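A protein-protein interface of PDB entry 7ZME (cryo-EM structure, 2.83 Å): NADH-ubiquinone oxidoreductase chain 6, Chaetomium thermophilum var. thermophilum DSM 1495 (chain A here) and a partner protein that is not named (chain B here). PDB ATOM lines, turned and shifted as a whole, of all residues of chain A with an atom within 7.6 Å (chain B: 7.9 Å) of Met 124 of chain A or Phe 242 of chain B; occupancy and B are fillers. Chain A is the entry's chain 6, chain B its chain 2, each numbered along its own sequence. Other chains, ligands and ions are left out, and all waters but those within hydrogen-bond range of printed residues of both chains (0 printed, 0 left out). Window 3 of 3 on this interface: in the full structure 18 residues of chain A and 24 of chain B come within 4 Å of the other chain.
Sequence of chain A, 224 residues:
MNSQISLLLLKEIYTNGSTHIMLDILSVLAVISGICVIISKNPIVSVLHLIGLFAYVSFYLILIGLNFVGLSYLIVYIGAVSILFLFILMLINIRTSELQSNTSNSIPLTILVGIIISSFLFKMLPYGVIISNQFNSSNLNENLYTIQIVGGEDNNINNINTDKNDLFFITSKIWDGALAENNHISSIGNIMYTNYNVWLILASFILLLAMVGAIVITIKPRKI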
ATOM      1  N   ILE A 116     -23.926   8.980  -7.699  1.00  0.00           N
ATOM      2  CA  ILE A 116     -24.380   7.700  -8.237  1.00  0.00           C
ATOM      3  C   ILE A 116     -23.356   6.606  -7.958  1.00  0.00           C
ATOM      4  O   ILE A 116     -23.697   5.534  -7.448  1.00  0.00           O
ATOM      5  CB  ILE A 116     -24.678   7.826  -9.741  1.00  0.00           C
ATOM      6  CG1 ILE A 116     -25.975   8.607  -9.958  1.00  0.00           C
ATOM      7  CG2 ILE A 116     -24.764   6.454 -10.385  1.00  0.00           C
ATOM      8  CD1 ILE A 116     -26.222   8.994 -11.398  1.00  0.00           C
ATOM      9  N   ILE A 117     -22.087   6.861  -8.281  1.00  0.00           N
ATOM     10  CA  ILE A 117     -21.064   5.837  -8.099  1.00  0.00           C
ATOM     11  C   ILE A 117     -20.878   5.523  -6.620  1.00  0.00           C
ATOM     12  O   ILE A 117     -20.862   4.355  -6.218  1.00  0.00           O
ATOM     13  CB  ILE A 117     -19.741   6.270  -8.756  1.00  0.00           C
ATOM     14  CG1 ILE A 117     -19.951   6.584 -10.234  1.00  0.00           C
ATOM     15  CG2 ILE A 117     -18.717   5.177  -8.645  1.00  0.00           C
ATOM     16  CD1 ILE A 117     -18.662   6.784 -10.990  1.00  0.00           C
ATOM     17  N   SER A 118     -20.763   6.558  -5.786  1.00  0.00           N
ATOM     18  CA  SER A 118     -20.515   6.340  -4.365  1.00  0.00           C
ATOM     19  C   SER A 118     -21.663   5.589  -3.703  1.00  0.00           C
ATOM     20  O   SER A 118     -21.435   4.683  -2.895  1.00  0.00           O
ATOM     21  CB  SER A 118     -20.278   7.676  -3.664  1.00  0.00           C
ATOM     22  OG  SER A 118     -21.243   8.631  -4.059  1.00  0.00           O
ATOM     23  N   SER A 119     -22.904   5.962  -4.020  1.00  0.00           N
ATOM     24  CA  SER A 119     -24.046   5.242  -3.471  1.00  0.00           C
ATOM     25  C   SER A 119     -24.078   3.805  -3.970  1.00  0.00           C
ATOM     26  O   SER A 119     -24.338   2.875  -3.197  1.00  0.00           O
ATOM     27  CB  SER A 119     -25.344   5.965  -3.826  1.00  0.00           C
ATOM     28  OG  SER A 119     -26.455   5.088  -3.753  1.00  0.00           O
ATOM     29  N   PHE A 120     -23.805   3.604  -5.260  1.00  0.00           N
ATOM     30  CA  PHE A 120     -23.783   2.255  -5.812  1.00  0.00           C
ATOM     31  C   PHE A 120     -22.588   1.457  -5.317  1.00  0.00           C
ATOM     32  O   PHE A 120     -22.692   0.238  -5.141  1.00  0.00           O
ATOM     33  CB  PHE A 120     -23.781   2.314  -7.335  1.00  0.00           C
ATOM     34  CG  PHE A 120     -25.130   2.560  -7.923  1.00  0.00           C
ATOM     35  CD1 PHE A 120     -26.224   2.784  -7.105  1.00  0.00           C
ATOM     36  CD2 PHE A 120     -25.312   2.552  -9.288  1.00  0.00           C
ATOM     37  CE1 PHE A 120     -27.472   3.005  -7.643  1.00  0.00           C
ATOM     38  CE2 PHE A 120     -26.555   2.767  -9.831  1.00  0.00           C
ATOM     39  CZ  PHE A 120     -27.638   2.997  -9.011  1.00  0.00           C
ATOM     40  N   LEU A 121     -21.456   2.109  -5.092  1.00  0.00           N
ATOM     41  CA  LEU A 121     -20.252   1.406  -4.687  1.00  0.00           C
ATOM     42  C   LEU A 121     -20.144   1.251  -3.175  1.00  0.00           C
ATOM     43  O   LEU A 121     -19.110   0.789  -2.686  1.00  0.00           O
ATOM     44  CB  LEU A 121     -19.007   2.124  -5.215  1.00  0.00           C
ATOM     45  CG  LEU A 121     -18.468   1.892  -6.632  1.00  0.00           C
ATOM     46  CD1 LEU A 121     -17.182   2.679  -6.827  1.00  0.00           C
ATOM     47  CD2 LEU A 121     -18.250   0.438  -6.978  1.00  0.00           C
ATOM     48  N   PHE A 122     -21.175   1.637  -2.421  1.00  0.00           N
ATOM     49  CA  PHE A 122     -21.113   1.537  -0.967  1.00  0.00           C
ATOM     50  C   PHE A 122     -21.466   0.136  -0.484  1.00  0.00           C
ATOM     51  O   PHE A 122     -20.716  -0.467   0.289  1.00  0.00           O
ATOM     52  CB  PHE A 122     -22.041   2.567  -0.324  1.00  0.00           C
ATOM     53  CG  PHE A 122     -21.614   2.985   1.052  1.00  0.00           C
ATOM     54  CD1 PHE A 122     -20.493   3.778   1.238  1.00  0.00           C
ATOM     55  CD2 PHE A 122     -22.323   2.567   2.164  1.00  0.00           C
ATOM     56  CE1 PHE A 122     -20.100   4.159   2.507  1.00  0.00           C
ATOM     57  CE2 PHE A 122     -21.934   2.941   3.435  1.00  0.00           C
ATOM     58  CZ  PHE A 122     -20.821   3.738   3.607  1.00  0.00           C
ATOM     59  N   LYS A 123     -22.606  -0.403  -0.924  1.00  0.00           N
ATOM     60  CA  LYS A 123     -22.933  -1.779  -0.570  1.00  0.00           C
ATOM     61  C   LYS A 123     -21.996  -2.780  -1.224  1.00  0.00           C
ATOM     62  O   LYS A 123     -22.086  -3.976  -0.928  1.00  0.00           O
ATOM     63  CB  LYS A 123     -24.389  -2.101  -0.919  1.00  0.00           C
ATOM     64  CG  LYS A 123     -24.898  -1.534  -2.232  1.00  0.00           C
ATOM     65  CD  LYS A 123     -26.180  -2.243  -2.635  1.00  0.00           C
ATOM     66  CE  LYS A 123     -26.842  -1.578  -3.825  1.00  0.00           C
ATOM     67  NZ  LYS A 123     -27.537  -0.312  -3.446  1.00  0.00           N
ATOM     68  N   MET A 124     -21.098  -2.340  -2.084  1.00  0.00           N
ATOM     69  CA  MET A 124     -20.140  -3.330  -2.626  1.00  0.00           C
ATOM     70  C   MET A 124     -19.050  -3.577  -1.581  1.00  0.00           C
ATOM     71  O   MET A 124     -18.269  -4.502  -1.779  1.00  0.00           O
ATOM     72  CB  MET A 124     -19.528  -2.821  -3.935  1.00  0.00           C
ATOM     73  CG  MET A 124     -20.524  -2.183  -4.868  1.00  0.00           C
ATOM     74  SD  MET A 124     -20.183  -2.623  -6.586  1.00  0.00           S
ATOM     75  CE  MET A 124     -21.453  -1.694  -7.444  1.00  0.00           C
ATOM     76  N   LEU A 125     -19.018  -2.797  -0.499  1.00  0.00           N
ATOM     77  CA  LEU A 125     -17.959  -2.915   0.540  1.00  0.00           C
ATOM     78  C   LEU A 125     -18.492  -3.645   1.766  1.00  0.00           C
ATOM     79  O   LEU A 125     -19.664  -3.437   2.103  1.00  0.00           O
ATOM     80  CB  LEU A 125     -17.464  -1.521   0.911  1.00  0.00           C
ATOM     81  CG  LEU A 125     -16.076  -1.152   0.402  1.00  0.00           C
ATOM     82  CD1 LEU A 125     -16.092  -0.918  -1.099  1.00  0.00           C
ATOM     83  CD2 LEU A 125     -15.568   0.080   1.129  1.00  0.00           C
ATOM     84  N   PRO A 126     -17.680  -4.481   2.451  1.00  0.00           N
ATOM     85  CA  PRO A 126     -18.140  -5.319   3.569  1.00  0.00           C
ATOM     86  C   PRO A 126     -18.226  -4.642   4.943  1.00  0.00           C
ATOM     87  O   PRO A 126     -17.752  -3.532   5.074  1.00  0.00           O
ATOM     88  CB  PRO A 126     -17.065  -6.394   3.551  1.00  0.00           C
ATOM     89  CG  PRO A 126     -15.820  -5.596   3.328  1.00  0.00           C
ATOM     90  CD  PRO A 126     -16.237  -4.601   2.267  1.00  0.00           C
ATOM     91  N   ILE A 130     -16.945  -0.835   6.614  1.00  0.00           N
ATOM     92  CA  ILE A 130     -17.938   0.240   6.931  1.00  0.00           C
ATOM     93  C   ILE A 130     -18.062   0.465   8.444  1.00  0.00           C
ATOM     94  O   ILE A 130     -18.789   1.397   8.834  1.00  0.00           O
ATOM     95  CB  ILE A 130     -19.304  -0.042   6.273  1.00  0.00           C
ATOM     96  CG1 ILE A 130     -20.010  -1.249   6.896  1.00  0.00           C
ATOM     97  CG2 ILE A 130     -19.157  -0.188   4.767  1.00  0.00           C
ATOM     98  CD1 ILE A 130     -21.271  -1.657   6.173  1.00  0.00           C
ATOM     99  N   LEU B 192     -11.026  -3.208  -9.785  1.00  0.00           N
ATOM    100  CA  LEU B 192     -12.103  -2.985  -8.833  1.00  0.00           C
ATOM    101  C   LEU B 192     -13.051  -4.178  -8.798  1.00  0.00           C
ATOM    102  O   LEU B 192     -13.575  -4.535  -7.739  1.00  0.00           O
ATOM    103  CB  LEU B 192     -12.851  -1.700  -9.185  1.00  0.00           C
ATOM    104  CG  LEU B 192     -14.095  -1.357  -8.365  1.00  0.00           C
ATOM    105  CD1 LEU B 192     -13.746  -1.222  -6.897  1.00  0.00           C
ATOM    106  CD2 LEU B 192     -14.749  -0.093  -8.878  1.00  0.00           C
ATOM    107  N   GLY B 193     -13.278  -4.808  -9.952  1.00  0.00           N
ATOM    108  CA  GLY B 193     -14.132  -5.982  -9.989  1.00  0.00           C
ATOM    109  C   GLY B 193     -13.557  -7.151  -9.215  1.00  0.00           C
ATOM    110  O   GLY B 193     -14.262  -7.811  -8.450  1.00  0.00           O
ATOM    111  N   SER B 195     -11.215  -6.933  -6.859  1.00  0.00           N
ATOM    112  CA  SER B 195     -11.028  -6.562  -5.462  1.00  0.00           C
ATOM    113  C   SER B 195     -12.315  -6.733  -4.672  1.00  0.00           C
ATOM    114  O   SER B 195     -12.299  -7.252  -3.553  1.00  0.00           O
ATOM    115  CB  SER B 195     -10.523  -5.122  -5.361  1.00  0.00           C
ATOM    116  OG  SER B 195     -11.573  -4.194  -5.553  1.00  0.00           O
ATOM    117  N   LEU B 196     -13.444  -6.322  -5.242  1.00  0.00           N
ATOM    118  CA  LEU B 196     -14.708  -6.456  -4.529  1.00  0.00           C
ATOM    119  C   LEU B 196     -15.102  -7.914  -4.356  1.00  0.00           C
ATOM    120  O   LEU B 196     -15.782  -8.258  -3.385  1.00  0.00           O
ATOM    121  CB  LEU B 196     -15.800  -5.686  -5.259  1.00  0.00           C
ATOM    122  CG  LEU B 196     -15.575  -4.180  -5.188  1.00  0.00           C
ATOM    123  CD1 LEU B 196     -16.467  -3.462  -6.168  1.00  0.00           C
ATOM    124  CD2 LEU B 196     -15.777  -3.674  -3.772  1.00  0.00           C
ATOM    125  N   LEU B 197     -14.690  -8.778  -5.281  1.00  0.00           N
ATOM    126  CA  LEU B 197     -14.941 -10.205  -5.125  1.00  0.00           C
ATOM    127  C   LEU B 197     -14.160 -10.771  -3.947  1.00  0.00           C
ATOM    128  O   LEU B 197     -14.714 -11.498  -3.115  1.00  0.00           O
ATOM    129  CB  LEU B 197     -14.581 -10.937  -6.416  1.00  0.00           C
ATOM    130  CG  LEU B 197     -15.648 -10.928  -7.508  1.00  0.00           C
ATOM    131  CD1 LEU B 197     -15.222 -11.803  -8.658  1.00  0.00           C
ATOM    132  CD2 LEU B 197     -16.992 -11.379  -6.956  1.00  0.00           C
ATOM    133  N   VAL B 199     -12.773  -9.032  -1.438  1.00  0.00           N
ATOM    134  CA  VAL B 199     -13.128  -8.335  -0.208  1.00  0.00           C
ATOM    135  C   VAL B 199     -14.406  -8.895   0.403  1.00  0.00           C
ATOM    136  O   VAL B 199     -14.555  -8.929   1.630  1.00  0.00           O
ATOM    137  CB  VAL B 199     -13.224  -6.821  -0.496  1.00  0.00           C
ATOM    138  CG1 VAL B 199     -13.874  -6.099   0.625  1.00  0.00           C
ATOM    139  CG2 VAL B 199     -11.831  -6.251  -0.684  1.00  0.00           C
ATOM    140  N   ASN B 200     -15.327  -9.370  -0.424  1.00  0.00           N
ATOM    141  CA  ASN B 200     -16.612  -9.829   0.083  1.00  0.00           C
ATOM    142  C   ASN B 200     -16.669 -11.332   0.300  1.00  0.00           C
ATOM    143  O   ASN B 200     -17.446 -11.798   1.136  1.00  0.00           O
ATOM    144  CB  ASN B 200     -17.726  -9.409  -0.873  1.00  0.00           C
ATOM    145  CG  ASN B 200     -18.348  -8.086  -0.498  1.00  0.00           C
ATOM    146  OD1 ASN B 200     -19.224  -8.028   0.357  1.00  0.00           O
ATOM    147  ND2 ASN B 200     -17.902  -7.017  -1.138  1.00  0.00           N
ATOM    148  N   LYS B 236     -26.757 -12.000   1.911  1.00  0.00           N
ATOM    149  CA  LYS B 236     -27.172 -12.382   0.571  1.00  0.00           C
ATOM    150  C   LYS B 236     -26.051 -12.090  -0.418  1.00  0.00           C
ATOM    151  O   LYS B 236     -25.406 -11.040  -0.333  1.00  0.00           O
ATOM    152  CB  LYS B 236     -28.437 -11.634   0.158  1.00  0.00           C
ATOM    153  CG  LYS B 236     -29.687 -12.090   0.896  1.00  0.00           C
ATOM    154  CD  LYS B 236     -30.949 -11.540   0.250  1.00  0.00           C
ATOM    155  CE  LYS B 236     -31.313 -10.175   0.810  1.00  0.00           C
ATOM    156  NZ  LYS B 236     -31.849 -10.262   2.195  1.00  0.00           N
ATOM    157  N   PRO B 237     -25.795 -12.985  -1.359  1.00  0.00           N
ATOM    158  CA  PRO B 237     -24.627 -12.869  -2.238  1.00  0.00           C
ATOM    159  C   PRO B 237     -24.833 -11.882  -3.382  1.00  0.00           C
ATOM    160  O   PRO B 237     -24.603 -12.197  -4.551  1.00  0.00           O
ATOM    161  CB  PRO B 237     -24.451 -14.302  -2.752  1.00  0.00           C
ATOM    162  CG  PRO B 237     -25.830 -14.870  -2.732  1.00  0.00           C
ATOM    163  CD  PRO B 237     -26.684 -14.080  -1.780  1.00  0.00           C
ATOM    164  N   TYR B 238     -25.284 -10.676  -3.040  1.00  0.00           N
ATOM    165  CA  TYR B 238     -25.482  -9.654  -4.058  1.00  0.00           C
ATOM    166  C   TYR B 238     -24.168  -9.266  -4.716  1.00  0.00           C
ATOM    167  O   TYR B 238     -24.128  -9.050  -5.930  1.00  0.00           O
ATOM    168  CB  TYR B 238     -26.146  -8.422  -3.449  1.00  0.00           C
ATOM    169  CG  TYR B 238     -27.642  -8.527  -3.302  1.00  0.00           C
ATOM    170  CD1 TYR B 238     -28.467  -8.545  -4.415  1.00  0.00           C
ATOM    171  CD2 TYR B 238     -28.231  -8.599  -2.048  1.00  0.00           C
ATOM    172  CE1 TYR B 238     -29.837  -8.639  -4.284  1.00  0.00           C
ATOM    173  CE2 TYR B 238     -29.601  -8.692  -1.907  1.00  0.00           C
ATOM    174  CZ  TYR B 238     -30.399  -8.712  -3.029  1.00  0.00           C
ATOM    175  OH  TYR B 238     -31.765  -8.803  -2.895  1.00  0.00           O
ATOM    176  N   TYR B 239     -23.085  -9.219  -3.941  1.00  0.00           N
ATOM    177  CA  TYR B 239     -21.823  -8.684  -4.433  1.00  0.00           C
ATOM    178  C   TYR B 239     -21.333  -9.414  -5.671  1.00  0.00           C
ATOM    179  O   TYR B 239     -20.649  -8.814  -6.504  1.00  0.00           O
ATOM    180  CB  TYR B 239     -20.765  -8.750  -3.333  1.00  0.00           C
ATOM    181  CG  TYR B 239     -20.355 -10.154  -2.953  1.00  0.00           C
ATOM    182  CD1 TYR B 239     -21.072 -10.877  -2.015  1.00  0.00           C
ATOM    183  CD2 TYR B 239     -19.245 -10.757  -3.532  1.00  0.00           C
ATOM    184  CE1 TYR B 239     -20.699 -12.151  -1.666  1.00  0.00           C
ATOM    185  CE2 TYR B 239     -18.864 -12.032  -3.186  1.00  0.00           C
ATOM    186  CZ  TYR B 239     -19.596 -12.723  -2.253  1.00  0.00           C
ATOM    187  OH  TYR B 239     -19.228 -13.999  -1.905  1.00  0.00           O
ATOM    188  N   LEU B 240     -21.673 -10.696  -5.821  1.00  0.00           N
ATOM    189  CA  LEU B 240     -21.125 -11.475  -6.925  1.00  0.00           C
ATOM    190  C   LEU B 240     -21.565 -10.920  -8.273  1.00  0.00           C
ATOM    191  O   LEU B 240     -20.732 -10.664  -9.149  1.00  0.00           O
ATOM    192  CB  LEU B 240     -21.529 -12.941  -6.787  1.00  0.00           C
ATOM    193  CG  LEU B 240     -21.308 -13.786  -8.042  1.00  0.00           C
ATOM    194  CD1 LEU B 240     -19.837 -14.133  -8.222  1.00  0.00           C
ATOM    195  CD2 LEU B 240     -22.146 -15.037  -7.977  1.00  0.00           C
ATOM    196  N   ASN B 241     -22.871 -10.714  -8.458  1.00  0.00           N
ATOM    197  CA  ASN B 241     -23.359 -10.236  -9.746  1.00  0.00           C
ATOM    198  C   ASN B 241     -22.845  -8.839 -10.066  1.00  0.00           C
ATOM    199  O   ASN B 241     -22.416  -8.575 -11.192  1.00  0.00           O
ATOM    200  CB  ASN B 241     -24.885 -10.262  -9.790  1.00  0.00           C
ATOM    201  CG  ASN B 241     -25.431 -11.617 -10.151  1.00  0.00           C
ATOM    202  OD1 ASN B 241     -24.909 -12.292 -11.032  1.00  0.00           O
ATOM    203  ND2 ASN B 241     -26.503 -12.014  -9.489  1.00  0.00           N
ATOM    204  N   PHE B 242     -22.882  -7.926  -9.105  1.00  0.00           N
ATOM    205  CA  PHE B 242     -22.437  -6.585  -9.440  1.00  0.00           C
ATOM    206  C   PHE B 242     -20.971  -6.302  -9.143  1.00  0.00           C
ATOM    207  O   PHE B 242     -20.516  -5.193  -9.432  1.00  0.00           O
ATOM    208  CB  PHE B 242     -23.355  -5.510  -8.823  1.00  0.00           C
ATOM    209  CG  PHE B 242     -23.420  -5.490  -7.326  1.00  0.00           C
ATOM    210  CD1 PHE B 242     -22.522  -4.786  -6.576  1.00  0.00           C
ATOM    211  CD2 PHE B 242     -24.370  -6.223  -6.669  1.00  0.00           C
ATOM    212  CE1 PHE B 242     -22.595  -4.771  -5.189  1.00  0.00           C
ATOM    213  CE2 PHE B 242     -24.454  -6.191  -5.294  1.00  0.00           C
ATOM    214  CZ  PHE B 242     -23.553  -5.482  -4.557  1.00  0.00           C
ATOM    215  N   SER B 243     -20.213  -7.252  -8.601  1.00  0.00           N
ATOM    216  CA  SER B 243     -18.768  -7.167  -8.797  1.00  0.00           C
ATOM    217  C   SER B 243     -18.385  -7.687 -10.173  1.00  0.00           C
ATOM    218  O   SER B 243     -17.469  -7.158 -10.810  1.00  0.00           O
ATOM    219  CB  SER B 243     -18.021  -7.935  -7.713  1.00  0.00           C
ATOM    220  OG  SER B 243     -18.477  -7.559  -6.432  1.00  0.00           O
ATOM    221  N   LEU B 244     -19.081  -8.722 -10.648  1.00  0.00           N
ATOM    222  CA  LEU B 244     -18.828  -9.254 -11.981  1.00  0.00           C
ATOM    223  C   LEU B 244     -19.309  -8.319 -13.077  1.00  0.00           C
ATOM    224  O   LEU B 244     -18.839  -8.428 -14.213  1.00  0.00           O
ATOM    225  CB  LEU B 244     -19.490 -10.624 -12.136  1.00  0.00           C
ATOM    226  CG  LEU B 244     -18.748 -11.815 -11.524  1.00  0.00           C
ATOM    227  CD1 LEU B 244     -19.507 -13.100 -11.765  1.00  0.00           C
ATOM    228  CD2 LEU B 244     -17.332 -11.914 -12.069  1.00  0.00           C
ATOM    229  N   LEU B 245     -20.235  -7.411 -12.764  1.00  0.00           N
ATOM    230  CA  LEU B 245     -20.687  -6.431 -13.744  1.00  0.00           C
ATOM    231  C   LEU B 245     -19.607  -5.393 -14.018  1.00  0.00           C
ATOM    232  O   LEU B 245     -19.336  -5.056 -15.173  1.00  0.00           O
ATOM    233  CB  LEU B 245     -21.966  -5.756 -13.252  1.00  0.00           C
ATOM    234  CG  LEU B 245     -22.564  -4.661 -14.136  1.00  0.00           C
ATOM    235  CD1 LEU B 245     -23.486  -5.263 -15.167  1.00  0.00           C
ATOM    236  CD2 LEU B 245     -23.296  -3.638 -13.300  1.00  0.00           C
ATOM    237  N   ILE B 246     -18.993  -4.863 -12.959  1.00  0.00           N
ATOM    238  CA  ILE B 246     -17.878  -3.935 -13.123  1.00  0.00           C
ATOM    239  C   ILE B 246     -16.704  -4.641 -13.783  1.00  0.00           C
ATOM    240  O   ILE B 246     -16.025  -4.084 -14.653  1.00  0.00           O
ATOM    241  CB  ILE B 246     -17.490  -3.336 -11.758  1.00  0.00           C
ATOM    242  CG1 ILE B 246     -18.610  -2.433 -11.246  1.00  0.00           C
ATOM    243  CG2 ILE B 246     -16.189  -2.562 -11.856  1.00  0.00           C
ATOM    244  CD1 ILE B 246     -18.669  -2.339  -9.756  1.00  0.00           C
ATOM    245  N   PHE B 247     -16.447  -5.878 -13.366  1.00  0.00           N
ATOM    246  CA  PHE B 247     -15.447  -6.719 -14.010  1.00  0.00           C
ATOM    247  C   PHE B 247     -15.725  -6.872 -15.501  1.00  0.00           C
ATOM    248  O   PHE B 247     -14.809  -6.781 -16.325  1.00  0.00           O
ATOM    249  CB  PHE B 247     -15.440  -8.073 -13.299  1.00  0.00           C
ATOM    250  CG  PHE B 247     -14.346  -9.003 -13.719  1.00  0.00           C
ATOM    251  CD1 PHE B 247     -13.098  -8.933 -13.134  1.00  0.00           C
ATOM    252  CD2 PHE B 247     -14.594 -10.006 -14.637  1.00  0.00           C
ATOM    253  CE1 PHE B 247     -12.104  -9.815 -13.496  1.00  0.00           C
ATOM    254  CE2 PHE B 247     -13.607 -10.893 -15.000  1.00  0.00           C
ATOM    255  CZ  PHE B 247     -12.357 -10.798 -14.427  1.00  0.00           C
ATOM    256  N   SER B 248     -16.991  -7.084 -15.868  1.00  0.00           N
ATOM    257  CA  SER B 248     -17.343  -7.311 -17.267  1.00  0.00           C
ATOM    258  C   SER B 248     -17.242  -6.041 -18.101  1.00  0.00           C
ATOM    259  O   SER B 248     -16.961  -6.113 -19.302  1.00  0.00           O
ATOM    260  CB  SER B 248     -18.753  -7.880 -17.362  1.00  0.00           C
ATOM    261  OG  SER B 248     -19.707  -6.936 -16.915  1.00  0.00           O
ATOM    262  N   PHE B 309     -30.500  -9.822 -11.172  1.00  0.00           N
ATOM    263  CA  PHE B 309     -29.388  -8.847 -11.194  1.00  0.00           C
ATOM    264  C   PHE B 309     -28.180  -9.430 -11.927  1.00  0.00           C
ATOM    265  O   PHE B 309     -27.065  -8.970 -11.653  1.00  0.00           O
ATOM    266  CB  PHE B 309     -29.020  -8.478  -9.757  1.00  0.00           C
ATOM    267  CG  PHE B 309     -30.119  -7.826  -8.960  1.00  0.00           C
ATOM    268  CD1 PHE B 309     -30.488  -6.513  -9.200  1.00  0.00           C
ATOM    269  CD2 PHE B 309     -30.774  -8.518  -7.956  1.00  0.00           C
ATOM    270  CE1 PHE B 309     -31.495  -5.912  -8.463  1.00  0.00           C
ATOM    271  CE2 PHE B 309     -31.784  -7.919  -7.222  1.00  0.00           C
ATOM    272  CZ  PHE B 309     -32.141  -6.615  -7.474  1.00  0.00           C
ATOM    273  N   SER B 310     -28.392 -10.353 -12.863  1.00  0.00           N
ATOM    274  CA  SER B 310     -27.244 -11.039 -13.502  1.00  0.00           C
ATOM    275  C   SER B 310     -26.325 -10.055 -14.218  1.00  0.00           C
ATOM    276  O   SER B 310     -26.826  -9.186 -14.932  1.00  0.00           O
ATOM    277  CB  SER B 310     -27.673 -12.142 -14.413  1.00  0.00           C
ATOM    278  OG  SER B 310     -26.555 -12.911 -14.823  1.00  0.00           O
ATOM    279  N   TRP B 311     -25.020 -10.232 -14.041  1.00  0.00           N
ATOM    280  CA  TRP B 311     -24.007  -9.375 -14.698  1.00  0.00           C
ATOM    281  C   TRP B 311     -24.069  -9.627 -16.199  1.00  0.00           C
ATOM    282  O   TRP B 311     -23.596  -8.774 -16.957  1.00  0.00           O
ATOM    283  CB  TRP B 311     -22.631  -9.721 -14.136  1.00  0.00           C
ATOM    284  CG  TRP B 311     -22.166 -11.104 -14.467  1.00  0.00           C
ATOM    285  CD1 TRP B 311     -22.497 -12.267 -13.837  1.00  0.00           C
ATOM    286  CD2 TRP B 311     -21.263 -11.464 -15.524  1.00  0.00           C
ATOM    287  NE1 TRP B 311     -21.867 -13.324 -14.433  1.00  0.00           N
ATOM    288  CE2 TRP B 311     -21.102 -12.861 -15.470  1.00  0.00           C
ATOM    289  CE3 TRP B 311     -20.588 -10.742 -16.513  1.00  0.00           C
ATOM    290  CZ2 TRP B 311     -20.296 -13.548 -16.371  1.00  0.00           C
ATOM    291  CZ3 TRP B 311     -19.784 -11.422 -17.399  1.00  0.00           C
ATOM    292  CH2 TRP B 311     -19.633 -12.804 -17.320  1.00  0.00           C
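Of the 23 printed residues of chain B, 5 touch a printed residue of chain A.
Printed residues of chain A that touch a printed residue of chain B: Leu 121, Met 124, Leu 125 and Pro 126.
Hydrophobic or aromatic side chains of chain A within 4 Å of the printed part of chain B: Leu 121, Met 124, Leu 125 and Pro 126.
Along chain A the printed residues that touch a printed residue of chain B span positions 121 to 126.
Among the printed residues, 7 pairs touch across the chains.
Leu 121 of chain A touches Ile 246 of chain B.
Leu 196 of chain B touches Met 124 of chain A.
Met 124 of chain A touches Phe 242 of chain B.
Met 124 of chain A touches Ile 246 of chain B.
Leu 196 of chain B touches Leu 125 of chain A (CD2 to CD1, 3.9 Å).
CG1 of Val 199 of chain B touches CD of Pro 126 of chain A, 3.2 Å away.
O of Leu 196 of chain B lies within hydrogen-bond range of ND2 of Asn 200 of chain B (3.3 Å).
Of the printed residues of chain B, Leu 121 of chain A touches Ile 246.
Met 124 of chain A touches just these residues of chain B: Leu 196, Asn 200, Phe 242 and Ile 246.
Of the printed residues of chain B, Leu 125 of chain A touches Leu 196 (3.9 Å).
Printed residues of chain A within 4 Å of Val 199 of chain B: Pro 126.
Of chain A, only Met 124 comes within 4 Å of Phe 242 of chain B.
Of the printed residues of chain A, Ile 246 of chain B touches Leu 121 (3.95 Å) and Met 124 (3.5 Å).
Phe 309 of chain B touches none of the printed residues of chain A.
The nearest residue of chain B that does not touch Met 124 of chain A is Ser 243 of chain B (5.0 Å).
The side-chain amide nitrogen of Asn 200 of chain B lies within hydrogen-bond range of the backbone carbonyl oxygen of Met 124 of chain A.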
